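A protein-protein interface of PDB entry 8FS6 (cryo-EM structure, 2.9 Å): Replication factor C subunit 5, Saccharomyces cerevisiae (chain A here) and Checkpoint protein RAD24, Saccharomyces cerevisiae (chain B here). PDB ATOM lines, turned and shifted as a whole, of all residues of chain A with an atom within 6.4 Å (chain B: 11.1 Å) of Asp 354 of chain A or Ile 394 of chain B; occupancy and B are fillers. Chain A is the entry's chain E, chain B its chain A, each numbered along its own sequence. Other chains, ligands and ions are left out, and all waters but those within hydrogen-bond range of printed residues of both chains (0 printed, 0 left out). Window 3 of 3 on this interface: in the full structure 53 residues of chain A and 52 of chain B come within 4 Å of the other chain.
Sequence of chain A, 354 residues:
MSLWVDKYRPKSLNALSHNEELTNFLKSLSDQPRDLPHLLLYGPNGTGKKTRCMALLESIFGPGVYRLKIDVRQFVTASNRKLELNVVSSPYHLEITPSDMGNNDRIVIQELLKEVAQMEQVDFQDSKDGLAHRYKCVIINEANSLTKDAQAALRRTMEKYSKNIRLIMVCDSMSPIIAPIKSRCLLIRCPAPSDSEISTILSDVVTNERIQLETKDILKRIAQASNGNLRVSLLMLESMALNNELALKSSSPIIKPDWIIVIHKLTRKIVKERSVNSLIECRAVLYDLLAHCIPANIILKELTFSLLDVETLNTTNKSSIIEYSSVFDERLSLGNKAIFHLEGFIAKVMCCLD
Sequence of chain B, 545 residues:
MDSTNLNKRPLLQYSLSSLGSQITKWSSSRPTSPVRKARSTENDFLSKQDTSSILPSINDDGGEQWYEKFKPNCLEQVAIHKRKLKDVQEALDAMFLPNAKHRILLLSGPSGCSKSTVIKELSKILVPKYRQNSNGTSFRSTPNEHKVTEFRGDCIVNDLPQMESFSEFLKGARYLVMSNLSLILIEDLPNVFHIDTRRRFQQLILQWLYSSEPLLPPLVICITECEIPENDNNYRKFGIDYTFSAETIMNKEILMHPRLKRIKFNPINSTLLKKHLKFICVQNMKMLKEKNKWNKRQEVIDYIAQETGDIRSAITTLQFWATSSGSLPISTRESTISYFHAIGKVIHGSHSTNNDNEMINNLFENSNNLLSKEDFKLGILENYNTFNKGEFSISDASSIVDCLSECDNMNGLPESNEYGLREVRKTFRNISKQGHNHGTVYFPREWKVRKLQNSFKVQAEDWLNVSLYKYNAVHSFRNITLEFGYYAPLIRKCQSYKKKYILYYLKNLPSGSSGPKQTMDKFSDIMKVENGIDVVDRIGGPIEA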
ATOM      1  N   ARG A 274     -13.105 -11.419 -25.171  1.00  0.00           N
ATOM      2  CA  ARG A 274     -13.001 -10.596 -23.967  1.00  0.00           C
ATOM      3  C   ARG A 274     -13.988 -11.145 -22.941  1.00  0.00           C
ATOM      4  O   ARG A 274     -15.139 -10.703 -22.877  1.00  0.00           O
ATOM      5  CB  ARG A 274     -13.268  -9.127 -24.282  1.00  0.00           C
ATOM      6  CG  ARG A 274     -12.236  -8.491 -25.195  1.00  0.00           C
ATOM      7  CD  ARG A 274     -12.672  -7.106 -25.634  1.00  0.00           C
ATOM      8  NE  ARG A 274     -13.895  -7.143 -26.428  1.00  0.00           N
ATOM      9  CZ  ARG A 274     -13.930  -7.302 -27.743  1.00  0.00           C
ATOM     10  NH1 ARG A 274     -12.823  -7.445 -28.452  1.00  0.00           N
ATOM     11  NH2 ARG A 274     -15.107  -7.319 -28.363  1.00  0.00           N
ATOM     12  N   SER A 275     -13.535 -12.105 -22.140  1.00  0.00           N
ATOM     13  CA  SER A 275     -14.375 -12.724 -21.125  1.00  0.00           C
ATOM     14  C   SER A 275     -13.488 -13.205 -19.984  1.00  0.00           C
ATOM     15  O   SER A 275     -12.258 -13.125 -20.049  1.00  0.00           O
ATOM     16  CB  SER A 275     -15.200 -13.872 -21.718  1.00  0.00           C
ATOM     17  OG  SER A 275     -14.361 -14.867 -22.275  1.00  0.00           O
ATOM     18  N   VAL A 276     -14.130 -13.705 -18.926  1.00  0.00           N
ATOM     19  CA  VAL A 276     -13.387 -14.205 -17.773  1.00  0.00           C
ATOM     20  C   VAL A 276     -12.636 -15.483 -18.131  1.00  0.00           C
ATOM     21  O   VAL A 276     -11.481 -15.670 -17.731  1.00  0.00           O
ATOM     22  CB  VAL A 276     -14.334 -14.415 -16.580  1.00  0.00           C
ATOM     23  CG1 VAL A 276     -13.576 -14.982 -15.390  1.00  0.00           C
ATOM     24  CG2 VAL A 276     -15.011 -13.106 -16.207  1.00  0.00           C
ATOM     25  N   LEU A 279      -9.746 -14.613 -19.988  1.00  0.00           N
ATOM     26  CA  LEU A 279      -8.746 -14.083 -19.064  1.00  0.00           C
ATOM     27  C   LEU A 279      -7.986 -15.207 -18.366  1.00  0.00           C
ATOM     28  O   LEU A 279      -6.780 -15.090 -18.125  1.00  0.00           O
ATOM     29  CB  LEU A 279      -9.419 -13.161 -18.048  1.00  0.00           C
ATOM     30  CG  LEU A 279      -8.527 -12.432 -17.042  1.00  0.00           C
ATOM     31  CD1 LEU A 279      -7.369 -11.754 -17.747  1.00  0.00           C
ATOM     32  CD2 LEU A 279      -9.343 -11.412 -16.268  1.00  0.00           C
ATOM     33  N   ASN A 317      -8.905   3.474 -27.831  1.00  0.00           N
ATOM     34  CA  ASN A 317      -8.493   2.185 -27.285  1.00  0.00           C
ATOM     35  C   ASN A 317      -6.979   2.103 -27.145  1.00  0.00           C
ATOM     36  O   ASN A 317      -6.469   1.590 -26.145  1.00  0.00           O
ATOM     37  CB  ASN A 317      -9.013   1.049 -28.165  1.00  0.00           C
ATOM     38  CG  ASN A 317     -10.521   0.911 -28.106  1.00  0.00           C
ATOM     39  OD1 ASN A 317     -11.194   1.633 -27.370  1.00  0.00           O
ATOM     40  ND2 ASN A 317     -11.060  -0.023 -28.881  1.00  0.00           N
ATOM     41  N   ALA A 347      -6.804  -7.605 -18.052  1.00  0.00           N
ATOM     42  CA  ALA A 347      -8.210  -7.375 -17.739  1.00  0.00           C
ATOM     43  C   ALA A 347      -8.626  -5.944 -18.056  1.00  0.00           C
ATOM     44  O   ALA A 347      -9.732  -5.713 -18.560  1.00  0.00           O
ATOM     45  CB  ALA A 347      -8.479  -7.699 -16.270  1.00  0.00           C
ATOM     46  N   VAL A 349      -7.279  -4.020 -20.365  1.00  0.00           N
ATOM     47  CA  VAL A 349      -7.353  -3.936 -21.821  1.00  0.00           C
ATOM     48  C   VAL A 349      -8.651  -4.556 -22.327  1.00  0.00           C
ATOM     49  O   VAL A 349      -9.328  -3.995 -23.199  1.00  0.00           O
ATOM     50  CB  VAL A 349      -6.117  -4.599 -22.458  1.00  0.00           C
ATOM     51  CG1 VAL A 349      -6.339  -4.844 -23.942  1.00  0.00           C
ATOM     52  CG2 VAL A 349      -4.884  -3.737 -22.240  1.00  0.00           C
ATOM     53  N   MET A 350      -9.025  -5.716 -21.778  1.00  0.00           N
ATOM     54  CA  MET A 350     -10.265  -6.369 -22.190  1.00  0.00           C
ATOM     55  C   MET A 350     -11.480  -5.507 -21.872  1.00  0.00           C
ATOM     56  O   MET A 350     -12.423  -5.431 -22.669  1.00  0.00           O
ATOM     57  CB  MET A 350     -10.390  -7.735 -21.516  1.00  0.00           C
ATOM     58  CG  MET A 350      -9.513  -8.814 -22.121  1.00  0.00           C
ATOM     59  SD  MET A 350      -9.561 -10.346 -21.174  1.00  0.00           S
ATOM     60  CE  MET A 350      -8.647 -11.438 -22.256  1.00  0.00           C
ATOM     61  N   CYS A 351     -11.481  -4.857 -20.706  1.00  0.00           N
ATOM     62  CA  CYS A 351     -12.602  -4.001 -20.337  1.00  0.00           C
ATOM     63  C   CYS A 351     -12.666  -2.753 -21.210  1.00  0.00           C
ATOM     64  O   CYS A 351     -13.758  -2.294 -21.563  1.00  0.00           O
ATOM     65  CB  CYS A 351     -12.505  -3.618 -18.862  1.00  0.00           C
ATOM     66  SG  CYS A 351     -12.833  -4.980 -17.730  1.00  0.00           S
ATOM     67  N   CYS A 352     -11.510  -2.187 -21.564  1.00  0.00           N
ATOM     68  CA  CYS A 352     -11.506  -0.970 -22.368  1.00  0.00           C
ATOM     69  C   CYS A 352     -11.850  -1.238 -23.828  1.00  0.00           C
ATOM     70  O   CYS A 352     -12.434  -0.370 -24.486  1.00  0.00           O
ATOM     71  CB  CYS A 352     -10.145  -0.277 -22.270  1.00  0.00           C
ATOM     72  SG  CYS A 352      -8.920  -0.837 -23.476  1.00  0.00           S
ATOM     73  N   LEU A 353     -11.472  -2.413 -24.336  1.00  0.00           N
ATOM     74  CA  LEU A 353     -11.716  -2.739 -25.766  1.00  0.00           C
ATOM     75  C   LEU A 353     -13.222  -2.871 -26.006  1.00  0.00           C
ATOM     76  O   LEU A 353     -13.701  -2.347 -27.028  1.00  0.00           O
ATOM     77  CB  LEU A 353     -10.986  -4.037 -26.125  1.00  0.00           C
ATOM     78  CG  LEU A 353      -9.480  -3.911 -26.342  1.00  0.00           C
ATOM     79  CD1 LEU A 353      -8.934  -5.136 -27.060  1.00  0.00           C
ATOM     80  CD2 LEU A 353      -9.150  -2.646 -27.116  1.00  0.00           C
ATOM     81  N   ASP A 354     -13.935  -3.544 -25.097  1.00  0.00           N
ATOM     82  CA  ASP A 354     -15.401  -3.749 -25.263  1.00  0.00           C
ATOM     83  C   ASP A 354     -16.168  -2.657 -24.506  1.00  0.00           C
ATOM     84  O   ASP A 354     -17.334  -2.873 -24.182  1.00  0.00           O
ATOM     85  CB  ASP A 354     -15.827  -5.161 -24.847  1.00  0.00           C
ATOM     86  CG  ASP A 354     -15.571  -5.502 -23.388  1.00  0.00           C
ATOM     87  OD1 ASP A 354     -15.092  -4.621 -22.652  1.00  0.00           O
ATOM     88  OD2 ASP A 354     -15.850  -6.654 -23.002  1.00  0.00           O
ATOM     89  OXT ASP A 354     -15.570  -1.602 -24.257  1.00  0.00           O
ATOM     90  N   LEU B 381      -6.580 -14.983  -6.596  1.00  0.00           N
ATOM     91  CA  LEU B 381      -6.432 -14.743  -8.028  1.00  0.00           C
ATOM     92  C   LEU B 381      -6.663 -16.011  -8.842  1.00  0.00           C
ATOM     93  O   LEU B 381      -7.135 -15.937  -9.982  1.00  0.00           O
ATOM     94  CB  LEU B 381      -5.044 -14.172  -8.317  1.00  0.00           C
ATOM     95  CG  LEU B 381      -4.729 -13.775  -9.761  1.00  0.00           C
ATOM     96  CD1 LEU B 381      -5.264 -12.386 -10.060  1.00  0.00           C
ATOM     97  CD2 LEU B 381      -3.233 -13.847 -10.024  1.00  0.00           C
ATOM     98  N   TYR B 384     -10.960 -16.798  -8.118  1.00  0.00           N
ATOM     99  CA  TYR B 384     -12.072 -15.867  -8.278  1.00  0.00           C
ATOM    100  C   TYR B 384     -12.900 -16.155  -9.526  1.00  0.00           C
ATOM    101  O   TYR B 384     -14.014 -15.636  -9.647  1.00  0.00           O
ATOM    102  CB  TYR B 384     -11.557 -14.426  -8.313  1.00  0.00           C
ATOM    103  CG  TYR B 384     -11.026 -13.989  -9.659  1.00  0.00           C
ATOM    104  CD1 TYR B 384      -9.765 -14.378 -10.085  1.00  0.00           C
ATOM    105  CD2 TYR B 384     -11.780 -13.178 -10.501  1.00  0.00           C
ATOM    106  CE1 TYR B 384      -9.270 -13.983 -11.310  1.00  0.00           C
ATOM    107  CE2 TYR B 384     -11.292 -12.778 -11.730  1.00  0.00           C
ATOM    108  CZ  TYR B 384     -10.035 -13.184 -12.128  1.00  0.00           C
ATOM    109  OH  TYR B 384      -9.541 -12.790 -13.348  1.00  0.00           O
ATOM    110  N   ASN B 385     -12.391 -16.970 -10.447  1.00  0.00           N
ATOM    111  CA  ASN B 385     -13.126 -17.310 -11.658  1.00  0.00           C
ATOM    112  C   ASN B 385     -14.126 -18.439 -11.451  1.00  0.00           C
ATOM    113  O   ASN B 385     -14.831 -18.802 -12.399  1.00  0.00           O
ATOM    114  CB  ASN B 385     -12.150 -17.690 -12.775  1.00  0.00           C
ATOM    115  CG  ASN B 385     -11.372 -18.953 -12.463  1.00  0.00           C
ATOM    116  OD1 ASN B 385     -10.442 -18.940 -11.657  1.00  0.00           O
ATOM    117  ND2 ASN B 385     -11.749 -20.053 -13.103  1.00  0.00           N
ATOM    118  N   PHE B 387     -16.645 -18.346  -9.216  1.00  0.00           N
ATOM    119  CA  PHE B 387     -17.878 -17.850  -8.613  1.00  0.00           C
ATOM    120  C   PHE B 387     -19.097 -18.277  -9.423  1.00  0.00           C
ATOM    121  O   PHE B 387     -20.062 -18.828  -8.882  1.00  0.00           O
ATOM    122  CB  PHE B 387     -17.820 -16.326  -8.488  1.00  0.00           C
ATOM    123  CG  PHE B 387     -19.049 -15.720  -7.872  1.00  0.00           C
ATOM    124  CD1 PHE B 387     -19.351 -15.940  -6.539  1.00  0.00           C
ATOM    125  CD2 PHE B 387     -19.903 -14.936  -8.628  1.00  0.00           C
ATOM    126  CE1 PHE B 387     -20.481 -15.384  -5.970  1.00  0.00           C
ATOM    127  CE2 PHE B 387     -21.035 -14.378  -8.066  1.00  0.00           C
ATOM    128  CZ  PHE B 387     -21.324 -14.602  -6.736  1.00  0.00           C
ATOM    129  N   ASN B 388     -19.063 -18.034 -10.731  1.00  0.00           N
ATOM    130  CA  ASN B 388     -20.130 -18.426 -11.642  1.00  0.00           C
ATOM    131  C   ASN B 388     -19.616 -19.348 -12.741  1.00  0.00           C
ATOM    132  O   ASN B 388     -20.163 -19.370 -13.846  1.00  0.00           O
ATOM    133  CB  ASN B 388     -20.792 -17.192 -12.252  1.00  0.00           C
ATOM    134  CG  ASN B 388     -22.244 -17.055 -11.858  1.00  0.00           C
ATOM    135  OD1 ASN B 388     -22.951 -18.050 -11.705  1.00  0.00           O
ATOM    136  ND2 ASN B 388     -22.701 -15.819 -11.694  1.00  0.00           N
ATOM    137  N   GLY B 390     -16.953 -18.762 -14.235  1.00  0.00           N
ATOM    138  CA  GLY B 390     -16.503 -17.788 -15.206  1.00  0.00           C
ATOM    139  C   GLY B 390     -17.587 -16.923 -15.812  1.00  0.00           C
ATOM    140  O   GLY B 390     -17.275 -16.081 -16.664  1.00  0.00           O
ATOM    141  N   GLU B 391     -18.841 -17.094 -15.405  1.00  0.00           N
ATOM    142  CA  GLU B 391     -19.959 -16.367 -16.009  1.00  0.00           C
ATOM    143  C   GLU B 391     -20.330 -15.138 -15.178  1.00  0.00           C
ATOM    144  O   GLU B 391     -21.423 -15.031 -14.623  1.00  0.00           O
ATOM    145  CB  GLU B 391     -21.156 -17.296 -16.187  1.00  0.00           C
ATOM    146  CG  GLU B 391     -22.118 -16.868 -17.285  1.00  0.00           C
ATOM    147  CD  GLU B 391     -21.525 -17.006 -18.674  1.00  0.00           C
ATOM    148  OE1 GLU B 391     -20.617 -17.844 -18.855  1.00  0.00           O
ATOM    149  OE2 GLU B 391     -21.968 -16.277 -19.586  1.00  0.00           O
ATOM    150  N   PHE B 392     -19.395 -14.195 -15.104  1.00  0.00           N
ATOM    151  CA  PHE B 392     -19.651 -12.887 -14.517  1.00  0.00           C
ATOM    152  C   PHE B 392     -18.961 -11.821 -15.358  1.00  0.00           C
ATOM    153  O   PHE B 392     -18.164 -12.121 -16.252  1.00  0.00           O
ATOM    154  CB  PHE B 392     -19.199 -12.811 -13.048  1.00  0.00           C
ATOM    155  CG  PHE B 392     -17.790 -13.278 -12.808  1.00  0.00           C
ATOM    156  CD1 PHE B 392     -17.523 -14.611 -12.542  1.00  0.00           C
ATOM    157  CD2 PHE B 392     -16.737 -12.378 -12.819  1.00  0.00           C
ATOM    158  CE1 PHE B 392     -16.230 -15.041 -12.311  1.00  0.00           C
ATOM    159  CE2 PHE B 392     -15.443 -12.802 -12.587  1.00  0.00           C
ATOM    160  CZ  PHE B 392     -15.190 -14.135 -12.332  1.00  0.00           C
ATOM    161  N   SER B 393     -19.290 -10.564 -15.070  1.00  0.00           N
ATOM    162  CA  SER B 393     -18.820  -9.451 -15.883  1.00  0.00           C
ATOM    163  C   SER B 393     -17.308  -9.286 -15.777  1.00  0.00           C
ATOM    164  O   SER B 393     -16.703  -9.521 -14.728  1.00  0.00           O
ATOM    165  CB  SER B 393     -19.513  -8.156 -15.462  1.00  0.00           C
ATOM    166  OG  SER B 393     -19.023  -7.051 -16.202  1.00  0.00           O
ATOM    167  N   ILE B 394     -16.698  -8.880 -16.892  1.00  0.00           N
ATOM    168  CA  ILE B 394     -15.258  -8.644 -16.908  1.00  0.00           C
ATOM    169  C   ILE B 394     -14.905  -7.367 -16.147  1.00  0.00           C
ATOM    170  O   ILE B 394     -13.787  -7.234 -15.636  1.00  0.00           O
ATOM    171  CB  ILE B 394     -14.745  -8.610 -18.361  1.00  0.00           C
ATOM    172  CG1 ILE B 394     -13.214  -8.594 -18.402  1.00  0.00           C
ATOM    173  CG2 ILE B 394     -15.322  -7.421 -19.118  1.00  0.00           C
ATOM    174  CD1 ILE B 394     -12.574  -9.827 -17.804  1.00  0.00           C
ATOM    175  N   SER B 395     -15.842  -6.418 -16.048  1.00  0.00           N
ATOM    176  CA  SER B 395     -15.598  -5.204 -15.278  1.00  0.00           C
ATOM    177  C   SER B 395     -15.435  -5.486 -13.790  1.00  0.00           C
ATOM    178  O   SER B 395     -14.793  -4.698 -13.089  1.00  0.00           O
ATOM    179  CB  SER B 395     -16.731  -4.200 -15.502  1.00  0.00           C
ATOM    180  OG  SER B 395     -17.929  -4.636 -14.884  1.00  0.00           O
ATOM    181  N   ASP B 396     -16.010  -6.582 -13.296  1.00  0.00           N
ATOM    182  CA  ASP B 396     -15.794  -7.027 -11.924  1.00  0.00           C
ATOM    183  C   ASP B 396     -14.471  -7.767 -11.769  1.00  0.00           C
ATOM    184  O   ASP B 396     -13.780  -7.608 -10.753  1.00  0.00           O
ATOM    185  CB  ASP B 396     -16.951  -7.923 -11.478  1.00  0.00           C
ATOM    186  N   ALA B 397     -14.099  -8.570 -12.768  1.00  0.00           N
ATOM    187  CA  ALA B 397     -12.806  -9.244 -12.733  1.00  0.00           C
ATOM    188  C   ALA B 397     -11.666  -8.235 -12.734  1.00  0.00           C
ATOM    189  O   ALA B 397     -10.675  -8.408 -12.017  1.00  0.00           O
ATOM    190  CB  ALA B 397     -12.679 -10.205 -13.914  1.00  0.00           C
ATOM    191  N   SER B 398     -11.788  -7.175 -13.536  1.00  0.00           N
ATOM    192  CA  SER B 398     -10.782  -6.119 -13.523  1.00  0.00           C
ATOM    193  C   SER B 398     -10.724  -5.417 -12.173  1.00  0.00           C
ATOM    194  O   SER B 398      -9.631  -5.121 -11.679  1.00  0.00           O
ATOM    195  CB  SER B 398     -11.062  -5.108 -14.634  1.00  0.00           C
ATOM    196  OG  SER B 398     -11.738  -3.970 -14.129  1.00  0.00           O
ATOM    197  N   SER B 399     -11.881  -5.144 -11.563  1.00  0.00           N
ATOM    198  CA  SER B 399     -11.915  -4.523 -10.244  1.00  0.00           C
ATOM    199  C   SER B 399     -11.365  -5.435  -9.154  1.00  0.00           C
ATOM    200  O   SER B 399     -11.004  -4.946  -8.078  1.00  0.00           O
ATOM    201  CB  SER B 399     -13.344  -4.108  -9.893  1.00  0.00           C
ATOM    202  OG  SER B 399     -13.930  -3.359 -10.944  1.00  0.00           O
ATOM    203  N   ILE B 400     -11.318  -6.742  -9.399  1.00  0.00           N
ATOM    204  CA  ILE B 400     -10.675  -7.644  -8.447  1.00  0.00           C
ATOM    205  C   ILE B 400      -9.164  -7.682  -8.665  1.00  0.00           C
ATOM    206  O   ILE B 400      -8.381  -7.523  -7.717  1.00  0.00           O
ATOM    207  CB  ILE B 400     -11.303  -9.046  -8.545  1.00  0.00           C
ATOM    208  CG1 ILE B 400     -12.724  -9.031  -7.977  1.00  0.00           C
ATOM    209  CG2 ILE B 400     -10.441 -10.075  -7.830  1.00  0.00           C
ATOM    210  CD1 ILE B 400     -13.444 -10.351  -8.099  1.00  0.00           C
ATOM    211  N   VAL B 401      -8.725  -7.890  -9.909  1.00  0.00           N
ATOM    212  CA  VAL B 401      -7.293  -8.010 -10.172  1.00  0.00           C
ATOM    213  C   VAL B 401      -6.534  -6.701  -9.978  1.00  0.00           C
ATOM    214  O   VAL B 401      -5.381  -6.735  -9.535  1.00  0.00           O
ATOM    215  CB  VAL B 401      -7.003  -8.565 -11.576  1.00  0.00           C
ATOM    216  CG1 VAL B 401      -5.580  -9.061 -11.639  1.00  0.00           C
ATOM    217  CG2 VAL B 401      -7.919  -9.727 -11.882  1.00  0.00           C
ATOM    218  N   ASP B 402      -7.125  -5.545 -10.292  1.00  0.00           N
ATOM    219  CA  ASP B 402      -6.396  -4.301 -10.067  1.00  0.00           C
ATOM    220  C   ASP B 402      -6.187  -4.031  -8.581  1.00  0.00           C
ATOM    221  O   ASP B 402      -5.122  -3.539  -8.192  1.00  0.00           O
ATOM    222  CB  ASP B 402      -7.109  -3.124 -10.749  1.00  0.00           C
ATOM    223  CG  ASP B 402      -8.378  -2.696 -10.034  1.00  0.00           C
ATOM    224  OD1 ASP B 402      -8.972  -3.516  -9.308  1.00  0.00           O
ATOM    225  OD2 ASP B 402      -8.783  -1.527 -10.203  1.00  0.00           O
ATOM    226  N   CYS B 403      -7.168  -4.367  -7.737  1.00  0.00           N
ATOM    227  CA  CYS B 403      -6.958  -4.257  -6.298  1.00  0.00           C
ATOM    228  C   CYS B 403      -5.926  -5.265  -5.809  1.00  0.00           C
ATOM    229  O   CYS B 403      -5.093  -4.932  -4.957  1.00  0.00           O
ATOM    230  CB  CYS B 403      -8.274  -4.450  -5.543  1.00  0.00           C
ATOM    231  SG  CYS B 403      -8.630  -6.161  -5.079  1.00  0.00           S
ATOM    232  N   THR B 427     -17.179  -7.130  -4.298  1.00  0.00           N
ATOM    233  CA  THR B 427     -17.448  -7.355  -5.713  1.00  0.00           C
ATOM    234  C   THR B 427     -18.308  -8.595  -5.923  1.00  0.00           C
ATOM    235  O   THR B 427     -19.247  -8.580  -6.728  1.00  0.00           O
ATOM    236  CB  THR B 427     -16.128  -7.480  -6.475  1.00  0.00           C
ATOM    237  OG1 THR B 427     -15.379  -6.265  -6.339  1.00  0.00           O
ATOM    238  CG2 THR B 427     -16.380  -7.746  -7.945  1.00  0.00           C
ATOM    239  N   PHE B 428     -18.013  -9.675  -5.200  1.00  0.00           N
ATOM    240  CA  PHE B 428     -18.795 -10.896  -5.343  1.00  0.00           C
ATOM    241  C   PHE B 428     -20.131 -10.832  -4.614  1.00  0.00           C
ATOM    242  O   PHE B 428     -21.018 -11.640  -4.905  1.00  0.00           O
ATOM    243  CB  PHE B 428     -17.986 -12.097  -4.852  1.00  0.00           C
ATOM    244  CG  PHE B 428     -16.982 -12.593  -5.850  1.00  0.00           C
ATOM    245  CD1 PHE B 428     -17.277 -12.588  -7.204  1.00  0.00           C
ATOM    246  CD2 PHE B 428     -15.744 -13.054  -5.440  1.00  0.00           C
ATOM    247  CE1 PHE B 428     -16.359 -13.039  -8.129  1.00  0.00           C
ATOM    248  CE2 PHE B 428     -14.820 -13.507  -6.362  1.00  0.00           C
ATOM    249  CZ  PHE B 428     -15.128 -13.499  -7.707  1.00  0.00           C
ATOM    250  N   ILE B 431     -22.808  -8.922  -6.987  1.00  0.00           N
ATOM    251  CA  ILE B 431     -23.292  -9.738  -8.092  1.00  0.00           C
ATOM    252  C   ILE B 431     -23.838 -11.076  -7.597  1.00  0.00           C
ATOM    253  O   ILE B 431     -23.994 -12.011  -8.380  1.00  0.00           O
ATOM    254  CB  ILE B 431     -22.199  -9.940  -9.154  1.00  0.00           C
ATOM    255  CG1 ILE B 431     -21.034 -10.746  -8.575  1.00  0.00           C
ATOM    256  CG2 ILE B 431     -21.712  -8.597  -9.679  1.00  0.00           C
ATOM    257  CD1 ILE B 431     -19.895 -10.961  -9.547  1.00  0.00           C
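Among the printed residues, merely in contact across the chains: Val 276 of chain A with Gly 390 of chain B (3.4 Å), Val 276 of chain A with Phe 392 of chain B (3.3 Å), Leu 279 of chain A with Tyr 384 of chain B (3.2 Å), Leu 279 of chain A with Ile 394 of chain B (3.9 Å), Ala 347 of chain A with Ser 398 of chain B (3.9 Å), Cys 351 of chain A with Ser 398 of chain B (3.6 Å) and Asp 354 of chain A with Ile 394 of chain B (3.99 Å).
Of the printed residues of chain B, Asp 354 of chain A touches Ile 394 (3.99 Å).
No residue of chain B comes within 4 Å of Met 350 of chain A.
No residue of chain B comes within 4 Å of Cys 352 of chain A.
No residue of chain B comes within 4 Å of Leu 353 of chain A.
Printed residues of chain A within 4 Å of Gly 390 of chain B: Val 276 (3.4 Å).
Of the printed residues of chain A, Phe 392 of chain B touches Val 276.
Ser 393 of chain B touches none of the printed residues of chain A.
The nearest printed residue of chain B that does not touch Asp 354 of chain A is Ser 395 of chain B (6.9 Å).
The nearest printed residue of chain A that does not touch Ile 394 of chain B is Ser 275 of chain A (4.002 Å).
The side-chain sulfur (SG) of Cys 351 of chain A lies within hydrogen-bond range of the backbone carbonyl oxygen (O) of Ile 394 of chain B (3.2 Å).
N of Ser 395 of chain B lies close to SG of Cys 351 of chain A, 3.7 Å away.
The backbone carbonyl oxygen of Asn 385 of chain B is in hydrogen-bond range of the backbone NH of Gly 390 of chain B, at 2.8 Å.
OG of Ser 395 of chain B is in hydrogen-bond range of OG of Ser 393 of chain B (3.0 Å).
The backbone carbonyl oxygen (O) of Ser 395 of chain B is in hydrogen-bond range of the side-chain hydroxyl (OG) of Ser 398 of chain B (3.3 Å).
OG of Ser 399 of chain B is in hydrogen-bond range of O of Ser 395 of chain B.
The guanidinium group (NE) of Arg 274 of chain A lies within salt-bridge range of the side-chain carboxylate (OD2) of Asp 354 of chain A (3.97 Å).
The backbone carbonyl oxygen of Ala 347 of chain A is in hydrogen-bond range of the side-chain sulfur of Cys 351 of chain A.
Hydrophobic or aromatic side chains of chain A that line the printed part of chain B: Val 276, Leu 279 and Ala 347.
Printed residues of chain B that touch a printed residue of chain A: Tyr 384, Gly 390, Phe 392, Ile 394, Ser 395 and Ser 398.
Hydrophobic or aromatic side chains of chain B within 4 Å of the printed part of chain A: Tyr 384, Phe 392 and Ile 394.
Among the printed residues, 9 pairs touch across the chains.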
